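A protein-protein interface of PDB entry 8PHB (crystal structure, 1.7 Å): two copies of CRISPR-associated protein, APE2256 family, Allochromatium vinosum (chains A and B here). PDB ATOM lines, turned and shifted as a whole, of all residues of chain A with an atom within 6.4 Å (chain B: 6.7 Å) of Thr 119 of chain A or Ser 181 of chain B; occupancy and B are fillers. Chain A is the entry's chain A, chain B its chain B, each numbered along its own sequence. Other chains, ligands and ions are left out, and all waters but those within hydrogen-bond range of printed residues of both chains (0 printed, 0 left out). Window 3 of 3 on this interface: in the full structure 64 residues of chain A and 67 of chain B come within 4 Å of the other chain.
The backbone NH (N) of Ser 181 of chain B sits at hydrogen-bond distance from the backbone carbonyl oxygen (O) of Val 118 of chain A (3.4 Å).
The backbone NH (N) of Gln 180 of chain B is in hydrogen-bond range of the backbone carbonyl oxygen (O) of Val 118 of chain A.
The backbone NH of Phe 178 of chain B sits at hydrogen-bond distance from the backbone carbonyl oxygen of Ala 183 of chain B (2.8 Å).
The backbone NH (N) of Ala 183 of chain B sits at hydrogen-bond distance from the side-chain hydroxyl (OG) of Ser 181 of chain B, at 3.1 Å.
The backbone carbonyl oxygen (O) of Phe 178 of chain B lies within hydrogen-bond range of the side-chain hydroxyl (OG) of Ser 181 of chain B.
The side-chain amide oxygen of Gln 117 of chain A is in hydrogen-bond range of the backbone NH of Thr 119 of chain A, at 3.0 Å.
The side-chain amide oxygen (OE1) of Gln 117 of chain A is in hydrogen-bond range of the backbone NH (N) of Asp 120 of chain A, at 2.7 Å.
Among the printed residues, merely in contact across the chains: Gln 117 of chain A with Phe 178 of chain B, Thr 119 of chain A with Ser 181 of chain B, Val 118 of chain A with Glu 179 of chain B, Ala 121 of chain A with Phe 178 of chain B, Ala 121 of chain A with Ala 183 of chain B, Asp 120 of chain A with Phe 178 of chain B, Ala 121 of chain A with Ile 185 of chain B and Val 118 of chain A with Phe 178 of chain B.
Of the printed residues of chain B, Thr 119 of chain A touches Ser 181.
Of the printed residues of chain A, Ser 181 of chain B touches Val 118 and Thr 119.
Printed residues of chain B within 4 Å of Ala 121 of chain A: Phe 178, Ala 183 and Ile 185.
Of the printed residues of chain B, Asp 120 of chain A touches Phe 178 (3.8 Å).
His 65 of chain B touches none of the printed residues of chain A.
The nearest printed residue of chain B that does not touch Thr 119 of chain A is Phe 178 of chain B (4.3 Å).
The nearest printed residue of chain A that does not touch Ser 181 of chain B is Ala 121 of chain A (4.2 Å).
No position is printed for both chains.
Of the 6 printed residues of chain A, 5 touch a printed residue of chain B.
Of the 11 printed residues of chain B, 6 touch a printed residue of chain A.
Printed residues of chain B that touch a printed residue of chain A: Phe 178, Glu 179, Gln 180, Ser 181, Ala 183 and Ile 185.
Among the printed residues, 10 pairs touch across the chains.
Among the printed residues, no Asp or Glu carboxylate lies within 4 Å of a Lys or Arg side-chain nitrogen of the other chain.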
ATOM      1  N   THR A  85      -4.337  23.925   9.853  1.00  0.00           N
ATOM      2  CA  THR A  85      -4.504  24.382  11.230  1.00  0.00           C
ATOM      3  C   THR A  85      -3.274  24.052  12.065  1.00  0.00           C
ATOM      4  O   THR A  85      -2.582  23.058  11.826  1.00  0.00           O
ATOM      5  CB  THR A  85      -5.743  23.731  11.869  1.00  0.00           C
ATOM      6  OG1 THR A  85      -5.538  22.315  11.994  1.00  0.00           O
ATOM      7  CG2 THR A  85      -6.975  23.945  11.009  1.00  0.00           C
ATOM      8  N   GLN A 117      -9.038  21.782   6.493  1.00  0.00           N
ATOM      9  CA  GLN A 117      -9.323  22.054   7.897  1.00  0.00           C
ATOM     10  C   GLN A 117     -10.694  21.453   8.188  1.00  0.00           C
ATOM     11  O   GLN A 117     -11.346  20.916   7.289  1.00  0.00           O
ATOM     12  CB  GLN A 117      -9.253  23.560   8.202  1.00  0.00           C
ATOM     13  CG  GLN A 117      -9.779  24.481   7.083  1.00  0.00           C
ATOM     14  CD  GLN A 117     -11.278  24.311   6.857  1.00  0.00           C
ATOM     15  OE1 GLN A 117     -12.057  24.378   7.804  1.00  0.00           O
ATOM     16  NE2 GLN A 117     -11.689  24.107   5.591  1.00  0.00           N
ATOM     17  N   VAL A 118     -11.115  21.498   9.456  1.00  0.00           N
ATOM     18  CA  VAL A 118     -12.259  20.679   9.857  1.00  0.00           C
ATOM     19  C   VAL A 118     -13.515  21.479  10.132  1.00  0.00           C
ATOM     20  O   VAL A 118     -14.531  20.879  10.504  1.00  0.00           O
ATOM     21  CB  VAL A 118     -11.925  19.800  11.077  1.00  0.00           C
ATOM     22  CG1 VAL A 118     -10.898  18.734  10.695  1.00  0.00           C
ATOM     23  CG2 VAL A 118     -11.460  20.668  12.239  1.00  0.00           C
ATOM     24  N   THR A 119     -13.512  22.789   9.928  1.00  0.00           N
ATOM     25  CA  THR A 119     -14.646  23.597  10.353  1.00  0.00           C
ATOM     26  C   THR A 119     -15.364  24.364   9.254  1.00  0.00           C
ATOM     27  O   THR A 119     -16.513  24.758   9.475  1.00  0.00           O
ATOM     28  CB  THR A 119     -14.207  24.614  11.415  1.00  0.00           C
ATOM     29  OG1 THR A 119     -13.172  25.429  10.870  1.00  0.00           O
ATOM     30  CG2 THR A 119     -13.683  23.898  12.645  1.00  0.00           C
ATOM     31  N   ASP A 120     -14.735  24.598   8.090  1.00  0.00           N
ATOM     32  CA  ASP A 120     -15.311  25.439   7.040  1.00  0.00           C
ATOM     33  C   ASP A 120     -15.499  24.558   5.809  1.00  0.00           C
ATOM     34  O   ASP A 120     -14.531  24.245   5.110  1.00  0.00           O
ATOM     35  CB  ASP A 120     -14.409  26.640   6.750  1.00  0.00           C
ATOM     36  CG  ASP A 120     -15.044  27.637   5.787  1.00  0.00           C
ATOM     37  OD1 ASP A 120     -15.792  27.209   4.872  1.00  0.00           O
ATOM     38  OD2 ASP A 120     -14.773  28.851   5.934  1.00  0.00           O
ATOM     39  N   ALA A 121     -16.747  24.148   5.556  1.00  0.00           N
ATOM     40  CA  ALA A 121     -17.020  23.236   4.455  1.00  0.00           C
ATOM     41  C   ALA A 121     -16.859  23.927   3.113  1.00  0.00           C
ATOM     42  O   ALA A 121     -16.553  23.268   2.110  1.00  0.00           O
ATOM     43  CB  ALA A 121     -18.435  22.675   4.563  1.00  0.00           C
ATOM     44  N   LYS B  57     -24.817  19.495  17.154  1.00  0.00           N
ATOM     45  CA  LYS B  57     -23.420  19.116  16.988  1.00  0.00           C
ATOM     46  C   LYS B  57     -22.877  18.351  18.187  1.00  0.00           C
ATOM     47  O   LYS B  57     -22.123  17.387  18.019  1.00  0.00           O
ATOM     48  CB  LYS B  57     -22.567  20.359  16.742  1.00  0.00           C
ATOM     49  N   HIS B  65     -27.897  14.386  13.273  1.00  0.00           N
ATOM     50  CA  HIS B  65     -27.369  15.655  12.796  1.00  0.00           C
ATOM     51  C   HIS B  65     -27.474  15.752  11.277  1.00  0.00           C
ATOM     52  O   HIS B  65     -27.995  16.733  10.731  1.00  0.00           O
ATOM     53  CB  HIS B  65     -25.915  15.777  13.249  1.00  0.00           C
ATOM     54  CG  HIS B  65     -25.281  17.091  12.922  1.00  0.00           C
ATOM     55  ND1 HIS B  65     -23.920  17.302  13.015  1.00  0.00           N
ATOM     56  CD2 HIS B  65     -25.819  18.267  12.517  1.00  0.00           C
ATOM     57  CE1 HIS B  65     -23.648  18.551  12.677  1.00  0.00           C
ATOM     58  NE2 HIS B  65     -24.784  19.161  12.386  1.00  0.00           N
ATOM     59  N   ILE B 177     -22.206  15.081   6.563  1.00  0.00           N
ATOM     60  CA  ILE B 177     -21.748  16.236   7.328  1.00  0.00           C
ATOM     61  C   ILE B 177     -20.238  16.305   7.222  1.00  0.00           C
ATOM     62  O   ILE B 177     -19.530  15.320   7.471  1.00  0.00           O
ATOM     63  CB  ILE B 177     -22.174  16.142   8.801  1.00  0.00           C
ATOM     64  CG1 ILE B 177     -23.700  16.228   8.949  1.00  0.00           C
ATOM     65  CG2 ILE B 177     -21.451  17.243   9.605  1.00  0.00           C
ATOM     66  CD1 ILE B 177     -24.290  17.619   8.828  1.00  0.00           C
ATOM     67  N   PHE B 178     -19.732  17.475   6.878  1.00  0.00           N
ATOM     68  CA  PHE B 178     -18.299  17.650   6.745  1.00  0.00           C
ATOM     69  C   PHE B 178     -17.641  17.839   8.104  1.00  0.00           C
ATOM     70  O   PHE B 178     -17.853  18.866   8.763  1.00  0.00           O
ATOM     71  CB  PHE B 178     -17.987  18.848   5.865  1.00  0.00           C
ATOM     72  CG  PHE B 178     -16.534  19.182   5.853  1.00  0.00           C
ATOM     73  CD1 PHE B 178     -15.627  18.293   5.293  1.00  0.00           C
ATOM     74  CD2 PHE B 178     -16.065  20.345   6.445  1.00  0.00           C
ATOM     75  CE1 PHE B 178     -14.274  18.584   5.281  1.00  0.00           C
ATOM     76  CE2 PHE B 178     -14.706  20.643   6.437  1.00  0.00           C
ATOM     77  CZ  PHE B 178     -13.813  19.753   5.881  1.00  0.00           C
ATOM     78  N   GLU B 179     -16.791  16.879   8.477  1.00  0.00           N
ATOM     79  CA  GLU B 179     -15.983  16.904   9.696  1.00  0.00           C
ATOM     80  C   GLU B 179     -16.703  17.596  10.853  1.00  0.00           C
ATOM     81  O   GLU B 179     -17.765  17.130  11.273  1.00  0.00           O
ATOM     82  CB  GLU B 179     -14.610  17.539   9.409  1.00  0.00           C
ATOM     83  CG  GLU B 179     -13.906  16.950   8.128  1.00  0.00           C
ATOM     84  CD  GLU B 179     -13.432  15.499   8.268  1.00  0.00           C
ATOM     85  OE1 GLU B 179     -12.944  15.166   9.369  1.00  0.00           O
ATOM     86  OE2 GLU B 179     -13.547  14.693   7.290  1.00  0.00           O
ATOM     87  N   GLN B 180     -16.088  18.622  11.433  1.00  0.00           N
ATOM     88  CA  GLN B 180     -16.629  19.248  12.631  1.00  0.00           C
ATOM     89  C   GLN B 180     -17.555  20.407  12.313  1.00  0.00           C
ATOM     90  O   GLN B 180     -17.964  21.132  13.228  1.00  0.00           O
ATOM     91  CB  GLN B 180     -15.496  19.713  13.550  1.00  0.00           C
ATOM     92  CG  GLN B 180     -15.341  18.850  14.788  1.00  0.00           C
ATOM     93  CD  GLN B 180     -16.609  18.804  15.615  1.00  0.00           C
ATOM     94  OE1 GLN B 180     -17.188  17.739  15.829  1.00  0.00           O
ATOM     95  NE2 GLN B 180     -17.049  19.965  16.089  1.00  0.00           N
ATOM     96  N   SER B 181     -17.884  20.605  11.040  1.00  0.00           N
ATOM     97  CA  SER B 181     -18.852  21.626  10.691  1.00  0.00           C
ATOM     98  C   SER B 181     -20.259  21.093  10.928  1.00  0.00           C
ATOM     99  O   SER B 181     -20.478  19.929  11.280  1.00  0.00           O
ATOM    100  CB  SER B 181     -18.677  22.063   9.238  1.00  0.00           C
ATOM    101  OG  SER B 181     -19.203  21.075   8.363  1.00  0.00           O
ATOM    102  N   SER B 182     -21.234  21.960  10.742  1.00  0.00           N
ATOM    103  CA  SER B 182     -22.621  21.533  10.704  1.00  0.00           C
ATOM    104  C   SER B 182     -23.149  21.614   9.283  1.00  0.00           C
ATOM    105  O   SER B 182     -24.328  21.899   9.068  1.00  0.00           O
ATOM    106  CB  SER B 182     -23.473  22.368  11.661  1.00  0.00           C
ATOM    107  OG  SER B 182     -24.502  21.581  12.246  1.00  0.00           O
ATOM    108  N   ALA B 183     -22.276  21.377   8.297  1.00  0.00           N
ATOM    109  CA  ALA B 183     -22.642  21.612   6.908  1.00  0.00           C
ATOM    110  C   ALA B 183     -22.517  20.307   6.143  1.00  0.00           C
ATOM    111  O   ALA B 183     -21.556  19.557   6.336  1.00  0.00           O
ATOM    112  CB  ALA B 183     -21.747  22.681   6.250  1.00  0.00           C
ATOM    113  N   LEU B 184     -23.504  20.035   5.296  1.00  0.00           N
ATOM    114  CA  LEU B 184     -23.447  18.909   4.383  1.00  0.00           C
ATOM    115  C   LEU B 184     -22.570  19.238   3.182  1.00  0.00           C
ATOM    116  O   LEU B 184     -22.507  20.383   2.731  1.00  0.00           O
ATOM    117  CB  LEU B 184     -24.840  18.571   3.871  1.00  0.00           C
ATOM    118  CG  LEU B 184     -25.846  17.991   4.837  1.00  0.00           C
ATOM    119  CD1 LEU B 184     -27.180  17.924   4.135  1.00  0.00           C
ATOM    120  CD2 LEU B 184     -25.394  16.609   5.288  1.00  0.00           C
ATOM    121  N   ILE B 185     -21.899  18.220   2.660  1.00  0.00           N
ATOM    122  CA  ILE B 185     -21.239  18.328   1.358  1.00  0.00           C
ATOM    123  C   ILE B 185     -21.612  17.084   0.557  1.00  0.00           C
ATOM    124  O   ILE B 185     -21.846  16.013   1.142  1.00  0.00           O
ATOM    125  CB  ILE B 185     -19.715  18.469   1.495  1.00  0.00           C
ATOM    126  CG1 ILE B 185     -19.129  17.281   2.248  1.00  0.00           C
ATOM    127  CG2 ILE B 185     -19.343  19.785   2.178  1.00  0.00           C
ATOM    128  CD1 ILE B 185     -17.623  17.300   2.357  1.00  0.00           C
